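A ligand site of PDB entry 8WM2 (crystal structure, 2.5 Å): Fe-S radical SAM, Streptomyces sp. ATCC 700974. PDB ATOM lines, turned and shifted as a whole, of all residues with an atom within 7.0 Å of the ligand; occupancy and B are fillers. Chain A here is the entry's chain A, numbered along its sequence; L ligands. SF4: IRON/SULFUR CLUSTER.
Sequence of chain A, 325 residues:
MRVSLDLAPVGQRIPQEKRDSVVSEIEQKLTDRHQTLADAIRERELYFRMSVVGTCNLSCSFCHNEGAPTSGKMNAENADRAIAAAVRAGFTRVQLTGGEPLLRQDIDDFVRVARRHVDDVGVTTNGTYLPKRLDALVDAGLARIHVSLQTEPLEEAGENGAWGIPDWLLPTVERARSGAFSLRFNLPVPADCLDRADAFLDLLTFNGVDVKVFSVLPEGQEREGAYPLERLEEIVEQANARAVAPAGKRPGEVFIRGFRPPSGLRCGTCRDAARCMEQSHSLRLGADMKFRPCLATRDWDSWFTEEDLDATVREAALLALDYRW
SG of Cys 267 is bound to FE1 of the ligand (2.2 Å). The side-chain sulfur of Cys 276 binds an iron atom (FE2) of the ligand. The side-chain sulfur (SG) of Cys 294 binds an iron atom (FE3) of the ligand, at 2.3 Å. An iron atom (FE4) of the ligand is bound by the side-chain sulfur (SG) of Cys 270.
The side-chain sulfur (SG) of Cys 267 lies close to the backbone NH (N) of Gly 264. The side-chain sulfur of Cys 294 sits close to the guanidinium group of Arg 266, 3.1 Å away. The backbone carbonyl oxygen of Cys 294 sits at hydrogen-bond distance from the guanidinium group of Arg 298 (2.6 Å). SG of Cys 270 sits close to N of Asp 272. The guanidinium group of Arg 266 lies within salt-bridge range of the side-chain carboxylate of Asp 322 (2.8 Å). NH2 of Arg 266 sits at hydrogen-bond distance from O of Leu 319 (3.1 Å). The side-chain hydroxyl (OG1) of Thr 297 is in hydrogen-bond range of the side-chain carboxylate (OD2) of Asp 272 (3.2 Å).
Pro 262 touches the ligand (CG to S3, 3.7 Å). NH2 of Arg 266 touches FE3 of the ligand (3.6 Å). Thr 297 touches the ligand. Seven residues have an atom within 4 Å of the ligand: Pro 262, Arg 266, Cys 267, Cys 270, Cys 276, Cys 294 and Thr 297.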
ATOM      1  N   PRO A 262     -11.727  26.668  12.021  1.00  0.00           N
ATOM      2  CA  PRO A 262     -13.147  26.754  11.636  1.00  0.00           C
ATOM      3  C   PRO A 262     -13.296  27.477  10.295  1.00  0.00           C
ATOM      4  O   PRO A 262     -12.563  28.425   9.999  1.00  0.00           O
ATOM      5  CB  PRO A 262     -13.778  27.558  12.776  1.00  0.00           C
ATOM      6  CG  PRO A 262     -12.644  28.367  13.317  1.00  0.00           C
ATOM      7  CD  PRO A 262     -11.429  27.497  13.200  1.00  0.00           C
ATOM      8  N   SER A 263     -14.254  27.010   9.502  1.00  0.00           N
ATOM      9  CA  SER A 263     -14.427  27.524   8.153  1.00  0.00           C
ATOM     10  C   SER A 263     -15.900  27.669   7.785  1.00  0.00           C
ATOM     11  O   SER A 263     -16.263  27.545   6.605  1.00  0.00           O
ATOM     12  CB  SER A 263     -13.723  26.635   7.130  1.00  0.00           C
ATOM     13  OG  SER A 263     -14.189  25.299   7.230  1.00  0.00           O
ATOM     14  N   GLY A 264     -16.760  27.925   8.765  1.00  0.00           N
ATOM     15  CA  GLY A 264     -18.157  28.188   8.483  1.00  0.00           C
ATOM     16  C   GLY A 264     -18.381  29.633   8.063  1.00  0.00           C
ATOM     17  O   GLY A 264     -17.470  30.459   8.020  1.00  0.00           O
ATOM     18  N   LEU A 265     -19.644  29.931   7.740  1.00  0.00           N
ATOM     19  CA  LEU A 265     -20.002  31.283   7.316  1.00  0.00           C
ATOM     20  C   LEU A 265     -19.779  32.288   8.438  1.00  0.00           C
ATOM     21  O   LEU A 265     -19.374  33.432   8.188  1.00  0.00           O
ATOM     22  CB  LEU A 265     -21.461  31.312   6.871  1.00  0.00           C
ATOM     23  CG  LEU A 265     -21.806  30.468   5.639  1.00  0.00           C
ATOM     24  CD1 LEU A 265     -23.306  30.236   5.558  1.00  0.00           C
ATOM     25  CD2 LEU A 265     -21.299  31.145   4.373  1.00  0.00           C
ATOM     26  N   ARG A 266     -20.033  31.893   9.686  1.00  0.00           N
ATOM     27  CA  ARG A 266     -19.883  32.811  10.803  1.00  0.00           C
ATOM     28  C   ARG A 266     -18.437  32.945  11.263  1.00  0.00           C
ATOM     29  O   ARG A 266     -18.107  33.933  11.928  1.00  0.00           O
ATOM     30  CB  ARG A 266     -20.735  32.341  11.977  1.00  0.00           C
ATOM     31  CG  ARG A 266     -22.192  32.131  11.652  1.00  0.00           C
ATOM     32  CD  ARG A 266     -22.803  31.259  12.722  1.00  0.00           C
ATOM     33  NE  ARG A 266     -22.033  30.016  12.793  1.00  0.00           N
ATOM     34  CZ  ARG A 266     -21.910  29.266  13.873  1.00  0.00           C
ATOM     35  NH1 ARG A 266     -22.527  29.562  15.007  1.00  0.00           N
ATOM     36  NH2 ARG A 266     -21.130  28.186  13.818  1.00  0.00           N
ATOM     37  N   CYS A 267     -17.580  31.978  10.936  1.00  0.00           N
ATOM     38  CA  CYS A 267     -16.246  31.934  11.531  1.00  0.00           C
ATOM     39  C   CYS A 267     -15.309  32.991  10.974  1.00  0.00           C
ATOM     40  O   CYS A 267     -14.307  33.317  11.613  1.00  0.00           O
ATOM     41  CB  CYS A 267     -15.647  30.539  11.340  1.00  0.00           C
ATOM     42  SG  CYS A 267     -16.852  29.209  11.579  1.00  0.00           S
ATOM     43  N   GLY A 268     -15.607  33.533   9.786  1.00  0.00           N
ATOM     44  CA  GLY A 268     -14.713  34.494   9.180  1.00  0.00           C
ATOM     45  C   GLY A 268     -14.566  35.768  10.003  1.00  0.00           C
ATOM     46  O   GLY A 268     -13.474  36.318  10.124  1.00  0.00           O
ATOM     47  N   THR A 269     -15.680  36.238  10.579  1.00  0.00           N
ATOM     48  CA  THR A 269     -15.690  37.445  11.392  1.00  0.00           C
ATOM     49  C   THR A 269     -16.006  37.161  12.859  1.00  0.00           C
ATOM     50  O   THR A 269     -16.470  38.059  13.562  1.00  0.00           O
ATOM     51  CB  THR A 269     -16.695  38.453  10.826  1.00  0.00           C
ATOM     52  OG1 THR A 269     -18.009  37.899  10.889  1.00  0.00           O
ATOM     53  CG2 THR A 269     -16.352  38.790   9.383  1.00  0.00           C
ATOM     54  N   CYS A 270     -15.777  35.931  13.314  1.00  0.00           N
ATOM     55  CA  CYS A 270     -16.012  35.593  14.722  1.00  0.00           C
ATOM     56  C   CYS A 270     -14.803  35.997  15.546  1.00  0.00           C
ATOM     57  O   CYS A 270     -13.674  35.573  15.281  1.00  0.00           O
ATOM     58  CB  CYS A 270     -16.278  34.100  14.869  1.00  0.00           C
ATOM     59  SG  CYS A 270     -16.528  33.532  16.581  1.00  0.00           S
ATOM     60  N   ARG A 271     -15.041  36.829  16.567  1.00  0.00           N
ATOM     61  CA  ARG A 271     -13.988  37.330  17.449  1.00  0.00           C
ATOM     62  C   ARG A 271     -13.273  36.223  18.206  1.00  0.00           C
ATOM     63  O   ARG A 271     -12.182  36.461  18.745  1.00  0.00           O
ATOM     64  CB  ARG A 271     -14.568  38.339  18.432  1.00  0.00           C
ATOM     65  N   ASP A 272     -13.829  35.016  18.260  1.00  0.00           N
ATOM     66  CA  ASP A 272     -13.227  33.909  19.004  1.00  0.00           C
ATOM     67  C   ASP A 272     -12.720  32.815  18.087  1.00  0.00           C
ATOM     68  O   ASP A 272     -12.480  31.690  18.546  1.00  0.00           O
ATOM     69  CB  ASP A 272     -14.239  33.341  20.000  1.00  0.00           C
ATOM     70  CG  ASP A 272     -14.646  34.360  21.048  1.00  0.00           C
ATOM     71  OD1 ASP A 272     -13.756  34.813  21.800  1.00  0.00           O
ATOM     72  OD2 ASP A 272     -15.837  34.718  21.111  1.00  0.00           O
ATOM     73  N   ALA A 273     -12.520  33.125  16.805  1.00  0.00           N
ATOM     74  CA  ALA A 273     -12.057  32.116  15.851  1.00  0.00           C
ATOM     75  C   ALA A 273     -10.693  31.560  16.222  1.00  0.00           C
ATOM     76  O   ALA A 273     -10.426  30.370  16.008  1.00  0.00           O
ATOM     77  CB  ALA A 273     -12.038  32.709  14.441  1.00  0.00           C
ATOM     78  N   ALA A 274      -9.808  32.405  16.768  1.00  0.00           N
ATOM     79  CA  ALA A 274      -8.491  31.931  17.161  1.00  0.00           C
ATOM     80  C   ALA A 274      -8.537  30.956  18.324  1.00  0.00           C
ATOM     81  O   ALA A 274      -7.601  30.177  18.497  1.00  0.00           O
ATOM     82  CB  ALA A 274      -7.597  33.116  17.521  1.00  0.00           C
ATOM     83  N   ARG A 275      -9.612  30.972  19.117  1.00  0.00           N
ATOM     84  CA  ARG A 275      -9.746  30.078  20.256  1.00  0.00           C
ATOM     85  C   ARG A 275     -10.729  28.940  19.983  1.00  0.00           C
ATOM     86  O   ARG A 275     -11.060  28.195  20.909  1.00  0.00           O
ATOM     87  CB  ARG A 275     -10.186  30.869  21.491  1.00  0.00           C
ATOM     88  N   CYS A 276     -11.185  28.799  18.746  1.00  0.00           N
ATOM     89  CA  CYS A 276     -12.087  27.710  18.367  1.00  0.00           C
ATOM     90  C   CYS A 276     -11.231  26.544  17.908  1.00  0.00           C
ATOM     91  O   CYS A 276     -10.901  26.418  16.726  1.00  0.00           O
ATOM     92  CB  CYS A 276     -13.058  28.166  17.289  1.00  0.00           C
ATOM     93  SG  CYS A 276     -14.233  26.896  16.781  1.00  0.00           S
ATOM     94  N   MET A 277     -10.864  25.672  18.841  1.00  0.00           N
ATOM     95  CA  MET A 277      -9.964  24.567  18.560  1.00  0.00           C
ATOM     96  C   MET A 277     -10.628  23.202  18.722  1.00  0.00           C
ATOM     97  O   MET A 277      -9.942  22.187  18.547  1.00  0.00           O
ATOM     98  CB  MET A 277      -8.732  24.669  19.464  1.00  0.00           C
ATOM     99  CG  MET A 277      -7.957  25.956  19.254  1.00  0.00           C
ATOM    100  SD  MET A 277      -7.084  26.509  20.732  1.00  0.00           S
ATOM    101  CE  MET A 277      -8.447  26.685  21.874  1.00  0.00           C
ATOM    102  N   HIS A 281     -17.193  18.309  17.056  1.00  0.00           N
ATOM    103  CA  HIS A 281     -18.240  19.312  17.158  1.00  0.00           C
ATOM    104  C   HIS A 281     -19.572  18.678  17.543  1.00  0.00           C
ATOM    105  O   HIS A 281     -19.828  17.498  17.278  1.00  0.00           O
ATOM    106  CB  HIS A 281     -18.392  20.068  15.834  1.00  0.00           C
ATOM    107  CG  HIS A 281     -17.236  20.967  15.528  1.00  0.00           C
ATOM    108  ND1 HIS A 281     -16.102  20.535  14.882  1.00  0.00           N
ATOM    109  CD2 HIS A 281     -17.047  22.287  15.784  1.00  0.00           C
ATOM    110  CE1 HIS A 281     -15.259  21.544  14.754  1.00  0.00           C
ATOM    111  NE2 HIS A 281     -15.808  22.620  15.290  1.00  0.00           N
ATOM    112  N   PRO A 293     -24.565  26.250  19.971  1.00  0.00           N
ATOM    113  CA  PRO A 293     -24.025  25.656  18.740  1.00  0.00           C
ATOM    114  C   PRO A 293     -22.511  25.715  18.682  1.00  0.00           C
ATOM    115  O   PRO A 293     -21.900  24.946  17.923  1.00  0.00           O
ATOM    116  CB  PRO A 293     -24.665  26.502  17.622  1.00  0.00           C
ATOM    117  CG  PRO A 293     -25.551  27.525  18.322  1.00  0.00           C
ATOM    118  CD  PRO A 293     -25.066  27.613  19.737  1.00  0.00           C
ATOM    119  N   CYS A 294     -21.888  26.583  19.466  1.00  0.00           N
ATOM    120  CA  CYS A 294     -20.444  26.723  19.500  1.00  0.00           C
ATOM    121  C   CYS A 294     -19.974  26.707  20.951  1.00  0.00           C
ATOM    122  O   CYS A 294     -20.727  26.987  21.878  1.00  0.00           O
ATOM    123  CB  CYS A 294     -19.977  28.023  18.832  1.00  0.00           C
ATOM    124  SG  CYS A 294     -20.669  28.375  17.199  1.00  0.00           S
ATOM    125  N   LEU A 295     -18.688  26.389  21.118  1.00  0.00           N
ATOM    126  CA  LEU A 295     -18.051  26.424  22.424  1.00  0.00           C
ATOM    127  C   LEU A 295     -17.270  27.708  22.670  1.00  0.00           C
ATOM    128  O   LEU A 295     -17.300  28.253  23.783  1.00  0.00           O
ATOM    129  CB  LEU A 295     -17.100  25.234  22.578  1.00  0.00           C
ATOM    130  CG  LEU A 295     -16.323  25.121  23.894  1.00  0.00           C
ATOM    131  CD1 LEU A 295     -17.260  24.855  25.058  1.00  0.00           C
ATOM    132  CD2 LEU A 295     -15.258  24.034  23.796  1.00  0.00           C
ATOM    133  N   ALA A 296     -16.583  28.222  21.645  1.00  0.00           N
ATOM    134  CA  ALA A 296     -15.672  29.340  21.865  1.00  0.00           C
ATOM    135  C   ALA A 296     -16.402  30.664  22.010  1.00  0.00           C
ATOM    136  O   ALA A 296     -15.880  31.590  22.632  1.00  0.00           O
ATOM    137  CB  ALA A 296     -14.656  29.407  20.719  1.00  0.00           C
ATOM    138  N   THR A 297     -17.612  30.778  21.456  1.00  0.00           N
ATOM    139  CA  THR A 297     -18.370  32.011  21.546  1.00  0.00           C
ATOM    140  C   THR A 297     -19.775  31.738  22.045  1.00  0.00           C
ATOM    141  O   THR A 297     -20.304  30.628  21.903  1.00  0.00           O
ATOM    142  CB  THR A 297     -18.442  32.724  20.183  1.00  0.00           C
ATOM    143  OG1 THR A 297     -18.898  34.075  20.384  1.00  0.00           O
ATOM    144  CG2 THR A 297     -19.392  32.008  19.232  1.00  0.00           C
ATOM    145  N   ARG A 298     -20.362  32.761  22.679  1.00  0.00           N
ATOM    146  CA  ARG A 298     -21.726  32.709  23.177  1.00  0.00           C
ATOM    147  C   ARG A 298     -22.692  33.492  22.297  1.00  0.00           C
ATOM    148  O   ARG A 298     -23.870  33.619  22.657  1.00  0.00           O
ATOM    149  CB  ARG A 298     -21.781  33.245  24.611  1.00  0.00           C
ATOM    150  CG  ARG A 298     -20.844  32.568  25.608  1.00  0.00           C
ATOM    151  CD  ARG A 298     -21.484  31.336  26.270  1.00  0.00           C
ATOM    152  NE  ARG A 298     -21.845  30.320  25.299  1.00  0.00           N
ATOM    153  CZ  ARG A 298     -20.993  29.483  24.712  1.00  0.00           C
ATOM    154  NH1 ARG A 298     -19.695  29.514  24.993  1.00  0.00           N
ATOM    155  NH2 ARG A 298     -21.436  28.604  23.824  1.00  0.00           N
ATOM    156  N   TRP A 300     -24.182  32.874  19.578  1.00  0.00           N
ATOM    157  CA  TRP A 300     -25.236  32.116  18.913  1.00  0.00           C
ATOM    158  C   TRP A 300     -26.061  31.264  19.867  1.00  0.00           C
ATOM    159  O   TRP A 300     -26.846  30.426  19.405  1.00  0.00           O
ATOM    160  CB  TRP A 300     -24.622  31.253  17.806  1.00  0.00           C
ATOM    161  CG  TRP A 300     -23.737  32.060  16.930  1.00  0.00           C
ATOM    162  CD1 TRP A 300     -22.372  32.078  16.936  1.00  0.00           C
ATOM    163  CD2 TRP A 300     -24.144  33.015  15.936  1.00  0.00           C
ATOM    164  NE1 TRP A 300     -21.906  32.969  16.004  1.00  0.00           N
ATOM    165  CE2 TRP A 300     -22.976  33.564  15.374  1.00  0.00           C
ATOM    166  CE3 TRP A 300     -25.383  33.452  15.470  1.00  0.00           C
ATOM    167  CZ2 TRP A 300     -23.011  34.517  14.370  1.00  0.00           C
ATOM    168  CZ3 TRP A 300     -25.418  34.405  14.465  1.00  0.00           C
ATOM    169  CH2 TRP A 300     -24.236  34.924  13.922  1.00  0.00           C
ATOM    170  N   LEU A 319     -27.131  26.127  13.095  1.00  0.00           N
ATOM    171  CA  LEU A 319     -25.931  26.887  13.403  1.00  0.00           C
ATOM    172  C   LEU A 319     -24.788  25.974  13.844  1.00  0.00           C
ATOM    173  O   LEU A 319     -23.617  26.308  13.646  1.00  0.00           O
ATOM    174  CB  LEU A 319     -26.224  27.926  14.477  1.00  0.00           C
ATOM    175  CG  LEU A 319     -27.164  29.067  14.064  1.00  0.00           C
ATOM    176  CD1 LEU A 319     -27.873  29.630  15.280  1.00  0.00           C
ATOM    177  CD2 LEU A 319     -26.376  30.169  13.362  1.00  0.00           C
ATOM    178  N   ALA A 320     -25.111  24.818  14.440  1.00  0.00           N
ATOM    179  CA  ALA A 320     -24.086  23.888  14.878  1.00  0.00           C
ATOM    180  C   ALA A 320     -23.321  23.277  13.710  1.00  0.00           C
ATOM    181  O   ALA A 320     -22.176  22.840  13.888  1.00  0.00           O
ATOM    182  CB  ALA A 320     -24.702  22.788  15.736  1.00  0.00           C
ATOM    183  N   ASP A 322     -22.382  25.013  11.131  1.00  0.00           N
ATOM    184  CA  ASP A 322     -21.623  26.079  10.478  1.00  0.00           C
ATOM    185  C   ASP A 322     -20.235  26.174  11.098  1.00  0.00           C
ATOM    186  O   ASP A 322     -19.947  27.019  11.952  1.00  0.00           O
ATOM    187  CB  ASP A 322     -22.374  27.402  10.564  1.00  0.00           C
ATOM    188  CG  ASP A 322     -21.784  28.460   9.660  1.00  0.00           C
ATOM    189  OD1 ASP A 322     -21.808  28.270   8.419  1.00  0.00           O
ATOM    190  OD2 ASP A 322     -21.308  29.482  10.176  1.00  0.00           O
ATOM    191  N   TYR A 323     -19.348  25.282  10.664  1.00  0.00           N
ATOM    192  CA  TYR A 323     -17.945  25.334  11.037  1.00  0.00           C
ATOM    193  C   TYR A 323     -17.085  24.716   9.946  1.00  0.00           C
ATOM    194  O   TYR A 323     -15.862  24.907   9.923  1.00  0.00           O
ATOM    195  CB  TYR A 323     -17.710  24.622  12.376  1.00  0.00           C
ATOM    196  CG  TYR A 323     -17.989  23.139  12.362  1.00  0.00           C
ATOM    197  CD1 TYR A 323     -17.017  22.221  11.968  1.00  0.00           C
ATOM    198  CD2 TYR A 323     -19.229  22.647  12.755  1.00  0.00           C
ATOM    199  CE1 TYR A 323     -17.273  20.875  11.957  1.00  0.00           C
ATOM    200  CE2 TYR A 323     -19.496  21.291  12.743  1.00  0.00           C
ATOM    201  CZ  TYR A 323     -18.514  20.405  12.347  1.00  0.00           C
ATOM    202  OH  TYR A 323     -18.765  19.053  12.329  1.00  0.00           O
HETATM  203 FE1  SF4 L   1     -17.178  29.531  13.781  1.00  0.00          FE
HETATM  204 FE2  SF4 L   1     -15.766  28.431  16.170  1.00  0.00          FE
HETATM  205 FE3  SF4 L   1     -18.687  29.023  16.319  1.00  0.00          FE
HETATM  206 FE4  SF4 L   1     -16.732  31.313  16.165  1.00  0.00          FE
HETATM  207  S1  SF4 L   1     -16.981  29.623  17.457  1.00  0.00           S
HETATM  208  S2  SF4 L   1     -18.437  30.710  15.044  1.00  0.00           S
HETATM  209  S3  SF4 L   1     -15.465  30.134  14.907  1.00  0.00           S
HETATM  210  S4  SF4 L   1     -17.472  27.831  15.032  1.00  0.00           S
